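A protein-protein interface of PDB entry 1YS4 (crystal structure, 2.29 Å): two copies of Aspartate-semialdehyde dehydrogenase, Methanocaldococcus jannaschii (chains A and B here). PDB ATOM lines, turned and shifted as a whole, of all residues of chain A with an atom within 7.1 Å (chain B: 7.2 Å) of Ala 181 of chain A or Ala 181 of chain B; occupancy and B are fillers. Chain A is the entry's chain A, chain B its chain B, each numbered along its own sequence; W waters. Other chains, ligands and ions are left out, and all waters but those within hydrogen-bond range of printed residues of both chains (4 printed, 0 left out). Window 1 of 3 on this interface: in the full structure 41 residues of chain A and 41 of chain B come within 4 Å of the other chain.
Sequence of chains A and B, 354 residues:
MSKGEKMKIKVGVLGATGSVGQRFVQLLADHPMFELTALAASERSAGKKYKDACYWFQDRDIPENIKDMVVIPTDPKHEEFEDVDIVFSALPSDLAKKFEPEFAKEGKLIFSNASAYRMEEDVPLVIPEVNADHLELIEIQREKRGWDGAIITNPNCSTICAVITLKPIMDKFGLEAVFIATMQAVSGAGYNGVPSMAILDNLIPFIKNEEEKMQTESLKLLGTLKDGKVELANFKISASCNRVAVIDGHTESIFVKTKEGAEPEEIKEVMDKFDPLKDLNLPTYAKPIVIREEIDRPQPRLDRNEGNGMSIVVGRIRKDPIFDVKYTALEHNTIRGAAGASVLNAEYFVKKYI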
ATOM      1  N   PHE A 179     -23.391  21.232   0.163  1.00  0.00           N
ATOM      2  CA  PHE A 179     -22.776  19.963  -0.200  1.00  0.00           C
ATOM      3  C   PHE A 179     -23.788  18.838  -0.050  1.00  0.00           C
ATOM      4  O   PHE A 179     -24.485  18.751   0.963  1.00  0.00           O
ATOM      5  CB  PHE A 179     -21.554  19.675   0.670  1.00  0.00           C
ATOM      6  CG  PHE A 179     -20.312  20.398   0.235  1.00  0.00           C
ATOM      7  CD1 PHE A 179     -19.593  19.967  -0.871  1.00  0.00           C
ATOM      8  CD2 PHE A 179     -19.858  21.507   0.940  1.00  0.00           C
ATOM      9  CE1 PHE A 179     -18.439  20.634  -1.274  1.00  0.00           C
ATOM     10  CE2 PHE A 179     -18.700  22.179   0.545  1.00  0.00           C
ATOM     11  CZ  PHE A 179     -17.990  21.740  -0.559  1.00  0.00           C
ATOM     12  N   ILE A 180     -23.870  17.980  -1.064  1.00  0.00           N
ATOM     13  CA  ILE A 180     -24.770  16.827  -1.022  1.00  0.00           C
ATOM     14  C   ILE A 180     -24.042  15.542  -1.424  1.00  0.00           C
ATOM     15  O   ILE A 180     -23.344  15.503  -2.437  1.00  0.00           O
ATOM     16  CB  ILE A 180     -26.027  17.024  -1.919  1.00  0.00           C
ATOM     17  CG1 ILE A 180     -26.702  18.371  -1.628  1.00  0.00           C
ATOM     18  CG2 ILE A 180     -27.024  15.874  -1.712  1.00  0.00           C
ATOM     19  CD1 ILE A 180     -27.572  18.885  -2.746  1.00  0.00           C
ATOM     20  N   ALA A 181     -24.199  14.505  -0.607  1.00  0.00           N
ATOM     21  CA  ALA A 181     -23.757  13.163  -0.963  1.00  0.00           C
ATOM     22  C   ALA A 181     -24.961  12.229  -0.918  1.00  0.00           C
ATOM     23  O   ALA A 181     -25.640  12.129   0.104  1.00  0.00           O
ATOM     24  CB  ALA A 181     -22.666  12.684  -0.025  1.00  0.00           C
ATOM     25  N   THR A 182     -25.230  11.558  -2.034  1.00  0.00           N
ATOM     26  CA  THR A 182     -26.430  10.743  -2.143  1.00  0.00           C
ATOM     27  C   THR A 182     -26.135   9.248  -2.091  1.00  0.00           C
ATOM     28  O   THR A 182     -25.054   8.795  -2.474  1.00  0.00           O
ATOM     29  CB  THR A 182     -27.228  11.041  -3.429  1.00  0.00           C
ATOM     30  OG1 THR A 182     -26.569  10.447  -4.554  1.00  0.00           O
ATOM     31  CG2 THR A 182     -27.399  12.548  -3.645  1.00  0.00           C
ATOM     32  N   MET A 183     -27.117   8.499  -1.602  1.00  0.00           N
ATOM     33  CA  MET A 183     -27.099   7.047  -1.644  1.00  0.00           C
ATOM     34  C   MET A 183     -28.407   6.621  -2.284  1.00  0.00           C
ATOM     35  O   MET A 183     -29.463   6.616  -1.645  1.00  0.00           O
ATOM     36  CB  MET A 183     -26.929   6.472  -0.246  1.00  0.00           C
ATOM     37  CG  MET A 183     -25.558   6.773   0.347  1.00  0.00           C
ATOM     38  SD  MET A 183     -25.505   6.652   2.276  1.00  0.00           S
ATOM     39  CE  MET A 183     -26.563   8.255   2.683  1.00  0.00           C
ATOM     40  N   GLN A 184     -28.323   6.282  -3.565  1.00  0.00           N
ATOM     41  CA  GLN A 184     -29.510   6.188  -4.400  1.00  0.00           C
ATOM     42  C   GLN A 184     -29.973   4.765  -4.664  1.00  0.00           C
ATOM     43  O   GLN A 184     -29.177   3.885  -4.984  1.00  0.00           O
ATOM     44  CB  GLN A 184     -29.311   6.968  -5.704  1.00  0.00           C
ATOM     45  CG  GLN A 184     -29.098   8.460  -5.456  1.00  0.00           C
ATOM     46  CD  GLN A 184     -29.004   9.299  -6.723  1.00  0.00           C
ATOM     47  OE1 GLN A 184     -28.217  10.245  -6.787  1.00  0.00           O
ATOM     48  NE2 GLN A 184     -29.809   8.969  -7.729  1.00  0.00           N
ATOM     49  N   MET A 214     -28.246  17.829 -10.403  1.00  0.00           N
ATOM     50  CA  MET A 214     -28.441  18.386  -9.064  1.00  0.00           C
ATOM     51  C   MET A 214     -27.861  19.787  -8.927  1.00  0.00           C
ATOM     52  O   MET A 214     -28.406  20.622  -8.208  1.00  0.00           O
ATOM     53  CB  MET A 214     -27.826  17.479  -8.001  1.00  0.00           C
ATOM     54  CG  MET A 214     -28.500  16.132  -7.879  1.00  0.00           C
ATOM     55  SD  MET A 214     -27.902  15.201  -6.286  1.00  0.00           S
ATOM     56  CE  MET A 214     -28.866  16.255  -4.968  1.00  0.00           C
ATOM     57  N   SER A 238     -22.499  21.570  -4.637  1.00  0.00           N
ATOM     58  CA  SER A 238     -21.629  20.473  -5.054  1.00  0.00           C
ATOM     59  C   SER A 238     -22.183  19.122  -4.603  1.00  0.00           C
ATOM     60  O   SER A 238     -22.421  18.904  -3.411  1.00  0.00           O
ATOM     61  CB  SER A 238     -20.215  20.665  -4.505  1.00  0.00           C
ATOM     62  OG  SER A 238     -19.356  19.642  -4.974  1.00  0.00           O
ATOM     63  N   ALA A 239     -22.374  18.222  -5.564  1.00  0.00           N
ATOM     64  CA  ALA A 239     -22.937  16.907  -5.292  1.00  0.00           C
ATOM     65  C   ALA A 239     -21.966  15.770  -5.579  1.00  0.00           C
ATOM     66  O   ALA A 239     -21.140  15.848  -6.493  1.00  0.00           O
ATOM     67  CB  ALA A 239     -24.229  16.703  -6.076  1.00  0.00           C
ATOM     68  N   SER A 240     -22.075  14.721  -4.770  1.00  0.00           N
ATOM     69  CA  SER A 240     -21.447  13.440  -5.050  1.00  0.00           C
ATOM     70  C   SER A 240     -22.527  12.373  -4.978  1.00  0.00           C
ATOM     71  O   SER A 240     -23.178  12.206  -3.942  1.00  0.00           O
ATOM     72  CB  SER A 240     -20.338  13.148  -4.048  1.00  0.00           C
ATOM     73  OG  SER A 240     -19.723  11.910  -4.340  1.00  0.00           O
ATOM     74  N   CYS A 241     -22.732  11.672  -6.089  1.00  0.00           N
ATOM     75  CA  CYS A 241     -23.825  10.712  -6.199  1.00  0.00           C
ATOM     76  C   CYS A 241     -23.343   9.270  -6.246  1.00  0.00           C
ATOM     77  O   CYS A 241     -22.312   8.963  -6.853  1.00  0.00           O
ATOM     78  CB  CYS A 241     -24.699  11.026  -7.411  1.00  0.00           C
ATOM     79  SG  CYS A 241     -25.470  12.650  -7.321  1.00  0.00           S
ATOM     80  N   ASN A 242     -24.101   8.396  -5.585  1.00  0.00           N
ATOM     81  CA  ASN A 242     -23.731   6.992  -5.430  1.00  0.00           C
ATOM     82  C   ASN A 242     -24.937   6.087  -5.537  1.00  0.00           C
ATOM     83  O   ASN A 242     -26.038   6.458  -5.127  1.00  0.00           O
ATOM     84  CB  ASN A 242     -23.063   6.739  -4.077  1.00  0.00           C
ATOM     85  CG  ASN A 242     -21.921   7.697  -3.788  1.00  0.00           C
ATOM     86  OD1 ASN A 242     -20.766   7.407  -4.088  1.00  0.00           O
ATOM     87  ND2 ASN A 242     -22.242   8.844  -3.193  1.00  0.00           N
ATOM     88  N   THR A 251     -31.424   8.493  -0.234  1.00  0.00           N
ATOM     89  CA  THR A 251     -30.966   9.107   1.003  1.00  0.00           C
ATOM     90  C   THR A 251     -29.850  10.092   0.677  1.00  0.00           C
ATOM     91  O   THR A 251     -28.955   9.790  -0.112  1.00  0.00           O
ATOM     92  CB  THR A 251     -30.472   8.052   2.017  1.00  0.00           C
ATOM     93  OG1 THR A 251     -31.468   7.035   2.173  1.00  0.00           O
ATOM     94  CG2 THR A 251     -30.208   8.684   3.371  1.00  0.00           C
ATOM     95  N   GLU A 252     -29.918  11.274   1.279  1.00  0.00           N
ATOM     96  CA  GLU A 252     -28.965  12.339   0.993  1.00  0.00           C
ATOM     97  C   GLU A 252     -28.371  12.912   2.273  1.00  0.00           C
ATOM     98  O   GLU A 252     -29.103  13.256   3.201  1.00  0.00           O
ATOM     99  CB  GLU A 252     -29.642  13.448   0.180  1.00  0.00           C
ATOM    100  CG  GLU A 252     -30.194  12.967  -1.154  1.00  0.00           C
ATOM    101  CD  GLU A 252     -30.772  14.075  -2.017  1.00  0.00           C
ATOM    102  OE1 GLU A 252     -30.807  15.241  -1.575  1.00  0.00           O
ATOM    103  OE2 GLU A 252     -31.198  13.765  -3.144  1.00  0.00           O
ATOM    104  N   SER A 253     -27.045  12.989   2.322  1.00  0.00           N
ATOM    105  CA  SER A 253     -26.353  13.705   3.390  1.00  0.00           C
ATOM    106  C   SER A 253     -26.124  15.137   2.920  1.00  0.00           C
ATOM    107  O   SER A 253     -25.398  15.376   1.951  1.00  0.00           O
ATOM    108  CB  SER A 253     -25.020  13.034   3.738  1.00  0.00           C
ATOM    109  OG  SER A 253     -25.218  11.764   4.331  1.00  0.00           O
ATOM    110  N   ILE A 254     -26.762  16.083   3.600  1.00  0.00           N
ATOM    111  CA  ILE A 254     -26.748  17.480   3.170  1.00  0.00           C
ATOM    112  C   ILE A 254     -26.046  18.361   4.209  1.00  0.00           C
ATOM    113  O   ILE A 254     -26.287  18.229   5.405  1.00  0.00           O
ATOM    114  CB  ILE A 254     -28.181  17.982   2.842  1.00  0.00           C
ATOM    115  CG1 ILE A 254     -28.826  17.076   1.775  1.00  0.00           C
ATOM    116  CG2 ILE A 254     -28.153  19.438   2.371  1.00  0.00           C
ATOM    117  CD1 ILE A 254     -30.300  17.335   1.484  1.00  0.00           C
ATOM    118  N   PHE A 255     -25.149  19.226   3.731  1.00  0.00           N
ATOM    119  CA  PHE A 255     -24.427  20.184   4.571  1.00  0.00           C
ATOM    120  C   PHE A 255     -24.717  21.581   4.024  1.00  0.00           C
ATOM    121  O   PHE A 255     -24.434  21.866   2.856  1.00  0.00           O
ATOM    122  CB  PHE A 255     -22.914  19.926   4.537  1.00  0.00           C
ATOM    123  CG  PHE A 255     -22.520  18.475   4.706  1.00  0.00           C
ATOM    124  CD1 PHE A 255     -22.096  17.993   5.944  1.00  0.00           C
ATOM    125  CD2 PHE A 255     -22.540  17.596   3.617  1.00  0.00           C
ATOM    126  CE1 PHE A 255     -21.714  16.660   6.101  1.00  0.00           C
ATOM    127  CE2 PHE A 255     -22.165  16.264   3.764  1.00  0.00           C
ATOM    128  CZ  PHE A 255     -21.751  15.796   5.008  1.00  0.00           C
ATOM    129  N   PHE B 179     -15.096  18.052   3.975  1.00  0.00           N
ATOM    130  CA  PHE B 179     -16.371  17.354   4.141  1.00  0.00           C
ATOM    131  C   PHE B 179     -16.233  15.896   3.723  1.00  0.00           C
ATOM    132  O   PHE B 179     -15.626  15.592   2.689  1.00  0.00           O
ATOM    133  CB  PHE B 179     -17.482  18.019   3.321  1.00  0.00           C
ATOM    134  CG  PHE B 179     -18.051  19.254   3.957  1.00  0.00           C
ATOM    135  CD1 PHE B 179     -18.931  19.160   5.033  1.00  0.00           C
ATOM    136  CD2 PHE B 179     -17.715  20.515   3.477  1.00  0.00           C
ATOM    137  CE1 PHE B 179     -19.459  20.308   5.625  1.00  0.00           C
ATOM    138  CE2 PHE B 179     -18.242  21.665   4.058  1.00  0.00           C
ATOM    139  CZ  PHE B 179     -19.116  21.561   5.133  1.00  0.00           C
ATOM    140  N   ILE B 180     -16.796  14.999   4.533  1.00  0.00           N
ATOM    141  CA  ILE B 180     -16.773  13.567   4.244  1.00  0.00           C
ATOM    142  C   ILE B 180     -18.138  12.942   4.503  1.00  0.00           C
ATOM    143  O   ILE B 180     -18.732  13.139   5.561  1.00  0.00           O
ATOM    144  CB  ILE B 180     -15.703  12.815   5.080  1.00  0.00           C
ATOM    145  CG1 ILE B 180     -14.325  13.471   4.930  1.00  0.00           C
ATOM    146  CG2 ILE B 180     -15.635  11.338   4.671  1.00  0.00           C
ATOM    147  CD1 ILE B 180     -13.429  13.289   6.130  1.00  0.00           C
ATOM    148  N   ALA B 181     -18.631  12.199   3.516  1.00  0.00           N
ATOM    149  CA  ALA B 181     -19.809  11.355   3.681  1.00  0.00           C
ATOM    150  C   ALA B 181     -19.397   9.911   3.432  1.00  0.00           C
ATOM    151  O   ALA B 181     -18.857   9.595   2.376  1.00  0.00           O
ATOM    152  CB  ALA B 181     -20.898  11.771   2.721  1.00  0.00           C
ATOM    153  N   THR B 182     -19.642   9.036   4.402  1.00  0.00           N
ATOM    154  CA  THR B 182     -19.201   7.647   4.280  1.00  0.00           C
ATOM    155  C   THR B 182     -20.343   6.687   3.962  1.00  0.00           C
ATOM    156  O   THR B 182     -21.490   6.907   4.352  1.00  0.00           O
ATOM    157  CB  THR B 182     -18.472   7.141   5.550  1.00  0.00           C
ATOM    158  OG1 THR B 182     -19.428   6.901   6.591  1.00  0.00           O
ATOM    159  CG2 THR B 182     -17.415   8.136   6.031  1.00  0.00           C
ATOM    160  N   MET B 183     -20.004   5.625   3.239  1.00  0.00           N
ATOM    161  CA  MET B 183     -20.895   4.491   3.043  1.00  0.00           C
ATOM    162  C   MET B 183     -20.157   3.247   3.527  1.00  0.00           C
ATOM    163  O   MET B 183     -19.272   2.719   2.846  1.00  0.00           O
ATOM    164  CB  MET B 183     -21.315   4.378   1.581  1.00  0.00           C
ATOM    165  CG  MET B 183     -22.221   5.507   1.131  1.00  0.00           C
ATOM    166  SD  MET B 183     -22.183   5.787  -0.793  1.00  0.00           S
ATOM    167  CE  MET B 183     -20.334   6.417  -0.929  1.00  0.00           C
ATOM    168  N   GLN B 184     -20.520   2.795   4.720  1.00  0.00           N
ATOM    169  CA  GLN B 184     -19.694   1.838   5.445  1.00  0.00           C
ATOM    170  C   GLN B 184     -20.226   0.413   5.446  1.00  0.00           C
ATOM    171  O   GLN B 184     -21.424   0.171   5.619  1.00  0.00           O
ATOM    172  CB  GLN B 184     -19.427   2.330   6.874  1.00  0.00           C
ATOM    173  CG  GLN B 184     -18.612   3.621   6.915  1.00  0.00           C
ATOM    174  CD  GLN B 184     -18.336   4.134   8.320  1.00  0.00           C
ATOM    175  OE1 GLN B 184     -18.480   5.324   8.586  1.00  0.00           O
ATOM    176  NE2 GLN B 184     -17.922   3.241   9.221  1.00  0.00           N
ATOM    177  N   MET B 214     -13.963  10.491  13.521  1.00  0.00           N
ATOM    178  CA  MET B 214     -13.381  11.057  12.304  1.00  0.00           C
ATOM    179  C   MET B 214     -12.973  12.517  12.473  1.00  0.00           C
ATOM    180  O   MET B 214     -11.938  12.938  11.964  1.00  0.00           O
ATOM    181  CB  MET B 214     -14.350  10.933  11.131  1.00  0.00           C
ATOM    182  CG  MET B 214     -14.632   9.507  10.699  1.00  0.00           C
ATOM    183  SD  MET B 214     -15.620   9.479   9.028  1.00  0.00           S
ATOM    184  CE  MET B 214     -14.176  10.028   7.832  1.00  0.00           C
ATOM    185  N   SER B 238     -15.880  17.991   8.800  1.00  0.00           N
ATOM    186  CA  SER B 238     -17.258  17.589   9.069  1.00  0.00           C
ATOM    187  C   SER B 238     -17.580  16.277   8.368  1.00  0.00           C
ATOM    188  O   SER B 238     -17.396  16.151   7.152  1.00  0.00           O
ATOM    189  CB  SER B 238     -18.243  18.671   8.626  1.00  0.00           C
ATOM    190  OG  SER B 238     -19.571  18.319   8.980  1.00  0.00           O
ATOM    191  N   ALA B 239     -18.063  15.311   9.144  1.00  0.00           N
ATOM    192  CA  ALA B 239     -18.364  13.981   8.631  1.00  0.00           C
ATOM    193  C   ALA B 239     -19.838  13.620   8.772  1.00  0.00           C
ATOM    194  O   ALA B 239     -20.521  14.060   9.705  1.00  0.00           O
ATOM    195  CB  ALA B 239     -17.495  12.936   9.321  1.00  0.00           C
ATOM    196  N   SER B 240     -20.314  12.820   7.825  1.00  0.00           N
ATOM    197  CA  SER B 240     -21.632  12.211   7.898  1.00  0.00           C
ATOM    198  C   SER B 240     -21.476  10.739   7.553  1.00  0.00           C
ATOM    199  O   SER B 240     -21.024  10.392   6.463  1.00  0.00           O
ATOM    200  CB  SER B 240     -22.600  12.895   6.937  1.00  0.00           C
ATOM    201  OG  SER B 240     -23.921  12.426   7.141  1.00  0.00           O
ATOM    202  N   CYS B 241     -21.839   9.875   8.494  1.00  0.00           N
ATOM    203  CA  CYS B 241     -21.549   8.457   8.367  1.00  0.00           C
ATOM    204  C   CYS B 241     -22.805   7.623   8.174  1.00  0.00           C
ATOM    205  O   CYS B 241     -23.848   7.893   8.777  1.00  0.00           O
ATOM    206  CB  CYS B 241     -20.744   7.966   9.566  1.00  0.00           C
ATOM    207  SG  CYS B 241     -19.128   8.759   9.698  1.00  0.00           S
ATOM    208  N   ASN B 242     -22.690   6.619   7.312  1.00  0.00           N
ATOM    209  CA  ASN B 242     -23.821   5.786   6.924  1.00  0.00           C
ATOM    210  C   ASN B 242     -23.418   4.333   6.784  1.00  0.00           C
ATOM    211  O   ASN B 242     -22.311   4.029   6.331  1.00  0.00           O
ATOM    212  CB  ASN B 242     -24.426   6.262   5.600  1.00  0.00           C
ATOM    213  CG  ASN B 242     -24.790   7.732   5.614  1.00  0.00           C
ATOM    214  OD1 ASN B 242     -25.910   8.097   5.955  1.00  0.00           O
ATOM    215  ND2 ASN B 242     -23.841   8.583   5.244  1.00  0.00           N
ATOM    216  N   THR B 251     -16.548   3.164   1.670  1.00  0.00           N
ATOM    217  CA  THR B 251     -16.452   4.145   0.592  1.00  0.00           C
ATOM    218  C   THR B 251     -16.743   5.535   1.148  1.00  0.00           C
ATOM    219  O   THR B 251     -17.686   5.713   1.922  1.00  0.00           O
ATOM    220  CB  THR B 251     -17.431   3.814  -0.554  1.00  0.00           C
ATOM    221  OG1 THR B 251     -17.254   2.450  -0.948  1.00  0.00           O
ATOM    222  CG2 THR B 251     -17.192   4.714  -1.766  1.00  0.00           C
ATOM    223  N   GLU B 252     -15.926   6.509   0.755  1.00  0.00           N
ATOM    224  CA  GLU B 252     -16.042   7.876   1.267  1.00  0.00           C
ATOM    225  C   GLU B 252     -16.084   8.915   0.152  1.00  0.00           C
ATOM    226  O   GLU B 252     -15.216   8.932  -0.727  1.00  0.00           O
ATOM    227  CB  GLU B 252     -14.881   8.192   2.216  1.00  0.00           C
ATOM    228  CG  GLU B 252     -14.788   7.243   3.406  1.00  0.00           C
ATOM    229  CD  GLU B 252     -13.687   7.597   4.384  1.00  0.00           C
ATOM    230  OE1 GLU B 252     -12.929   8.561   4.146  1.00  0.00           O
ATOM    231  OE2 GLU B 252     -13.577   6.891   5.402  1.00  0.00           O
ATOM    232  N   SER B 253     -17.105   9.767   0.192  1.00  0.00           N
ATOM    233  CA  SER B 253     -17.175  10.940  -0.671  1.00  0.00           C
ATOM    234  C   SER B 253     -16.499  12.093   0.060  1.00  0.00           C
ATOM    235  O   SER B 253     -16.972  12.533   1.110  1.00  0.00           O
ATOM    236  CB  SER B 253     -18.626  11.295  -1.003  1.00  0.00           C
ATOM    237  OG  SER B 253     -19.239  10.281  -1.774  1.00  0.00           O
ATOM    238  N   ILE B 254     -15.386  12.568  -0.492  1.00  0.00           N
ATOM    239  CA  ILE B 254     -14.550  13.563   0.187  1.00  0.00           C
ATOM    240  C   ILE B 254     -14.468  14.859  -0.626  1.00  0.00           C
ATOM    241  O   ILE B 254     -14.224  14.828  -1.829  1.00  0.00           O
ATOM    242  CB  ILE B 254     -13.132  12.992   0.508  1.00  0.00           C
ATOM    243  CG1 ILE B 254     -13.250  11.679   1.300  1.00  0.00           C
ATOM    244  CG2 ILE B 254     -12.291  14.001   1.293  1.00  0.00           C
ATOM    245  CD1 ILE B 254     -11.936  10.968   1.564  1.00  0.00           C
ATOM    246  N   PHE B 255     -14.699  15.985   0.046  1.00  0.00           N
ATOM    247  CA  PHE B 255     -14.646  17.316  -0.558  1.00  0.00           C
ATOM    248  C   PHE B 255     -13.603  18.132   0.202  1.00  0.00           C
ATOM    249  O   PHE B 255     -13.725  18.318   1.414  1.00  0.00           O
ATOM    250  CB  PHE B 255     -16.005  18.021  -0.457  1.00  0.00           C
ATOM    251  CG  PHE B 255     -17.187  17.165  -0.848  1.00  0.00           C
ATOM    252  CD1 PHE B 255     -17.762  17.288  -2.109  1.00  0.00           C
ATOM    253  CD2 PHE B 255     -17.742  16.256   0.056  1.00  0.00           C
ATOM    254  CE1 PHE B 255     -18.866  16.514  -2.471  1.00  0.00           C
ATOM    255  CE2 PHE B 255     -18.836  15.471  -0.297  1.00  0.00           C
ATOM    256  CZ  PHE B 255     -19.404  15.603  -1.562  1.00  0.00           C
HETATM  257  O   HOH W   1     -17.028  13.648  -3.125  1.00  0.00           O
HETATM  258  O   HOH W   2     -18.409   8.532  -3.636  1.00  0.00           O
HETATM  259  O   HOH W   3     -25.054  15.443   6.212  1.00  0.00           O
HETATM  260  O   HOH W   4     -27.087  10.451   5.718  1.00  0.00           O
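Of the 17 printed residues of chain B, 8 touch a printed residue of chain A. Printed residues of chain B that touch a printed residue of chain A: Phe 179, Ala 181, Met 183, Ser 238, Ser 240, Asn 242, Ser 253 and Phe 255. Hydrophobic or aromatic side chains of chain B that line the printed part of chain A: Phe 179, Ala 181, Met 183 and Phe 255. Of the 17 printed residues of chain A, 7 touch a printed residue of chain B. Printed residues of chain A that touch a printed residue of chain B: Phe 179, Ala 181, Met 183, Ser 240, Asn 242, Ser 253 and Phe 255. Among the printed residues, 14 pairs touch across the chains.
Phe 179 of chain B touches Phe 179 of chain A. Phe 179 of chain A touches Phe 255 of chain B (CD1 to CD1, 3.5 Å). Ala 181 of chain A touches Ala 181 of chain B. Met 183 of chain A touches Asn 242 of chain B. CB of Ser 240 of chain A touches CZ of Phe 255 of chain B, at 3.6 Å. Asn 242 of chain A touches Met 183 of chain B (OD1 to CE, 3.3 Å). ND2 of Asn 242 of chain A touches OG of Ser 253 of chain B (3.6 Å). Asn 242 of chain B touches Ser 253 of chain A. CD1 of Phe 255 of chain A touches CD1 of Phe 179 of chain B, 3.5 Å away. CE1 of Phe 255 of chain A touches OG of Ser 238 of chain B, 3.95 Å away.
Phe 179 of chain B touches its own counterpart, Phe 179 of chain A. Phe 179 of chain A touches Phe 255 of chain B, and with the chains exchanged Phe 255 of chain A touches Phe 179 of chain B. Ala 181 of chain A touches its own counterpart, Ala 181 of chain B. Met 183 of chain B touches its own counterpart, Met 183 of chain A. 17 positions are printed for both chains. Of the 14 pairs that touch across the chains among the printed residues, 13 have their exchanged pair printed and touching as well.
Water W4 lies within hydrogen-bond range of the side-chain amide oxygen of Asn 242 of chain B and the side-chain hydroxyl of Ser 253 of chain A. Water W2 lies within hydrogen-bond range of OD1 of Asn 242 of chain A (2.7 Å) and OG of Ser 253 of chain B (2.7 Å). Water W3 bridges O of Ile 254 of chain A and OG of Ser 240 of chain B. Water W1 lies within hydrogen-bond range of the backbone NH of Ile 254 of chain B (3.3 Å) and the side-chain hydroxyl of Ser 240 of chain A (3.4 Å).
Ala 181 of chain A touches one residue of chain B. Ala 181 of chain B touches just one residue of chain A: Ala 181. Of the printed residues of chain B, Phe 179 of chain A touches Phe 179 (3.5 Å) and Phe 255 (3.5 Å). Of the printed residues of chain A, Ser 238 of chain B touches Phe 255 (3.95 Å). Of the printed residues of chain A, Phe 179 of chain B touches Phe 179 (3.5 Å) and Phe 255 (3.5 Å). Of the printed residues of chain A, Phe 255 of chain B touches Phe 179 (3.5 Å) and Ser 240 (3.6 Å). Printed residues of chain B within 4 Å of Ser 253 of chain A: Ser 240 (3.2 Å) and Asn 242 (3.6 Å). Ile 180 of chain A touches none of the printed residues of chain B. The nearest residue of chain A that does not touch Ala 181 of chain B is Ser 253 of chain A (4.4 Å). The nearest printed residue of chain B that does not touch Phe 255 of chain A is Ile 180 of chain B (4.1 Å).
The backbone NH of Ser 240 of chain A sits at hydrogen-bond distance from the backbone carbonyl oxygen of Ile 180 of chain A (2.8 Å). The backbone carbonyl oxygen (O) of Ala 181 of chain A sits at hydrogen-bond distance from the backbone NH (N) of Ser 253 of chain A (2.8 Å). The backbone carbonyl oxygen (O) of Thr 251 of chain A lies within hydrogen-bond range of the backbone NH (N) of Met 183 of chain A. The backbone carbonyl oxygen (O) of Ile 180 of chain B sits at hydrogen-bond distance from the backbone NH (N) of Ser 240 of chain B (2.8 Å). O of Thr 251 of chain B lies within hydrogen-bond range of N of Met 183 of chain B (2.7 Å). N of Gln 184 of chain B is in hydrogen-bond range of O of Asn 242 of chain B (2.7 Å).
The side-chain hydroxyl (OG) of Ser 240 of chain A is in hydrogen-bond range of the side-chain hydroxyl (OG) of Ser 253 of chain B (3.1 Å). OG of Ser 240 of chain B sits at hydrogen-bond distance from OG of Ser 253 of chain A.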
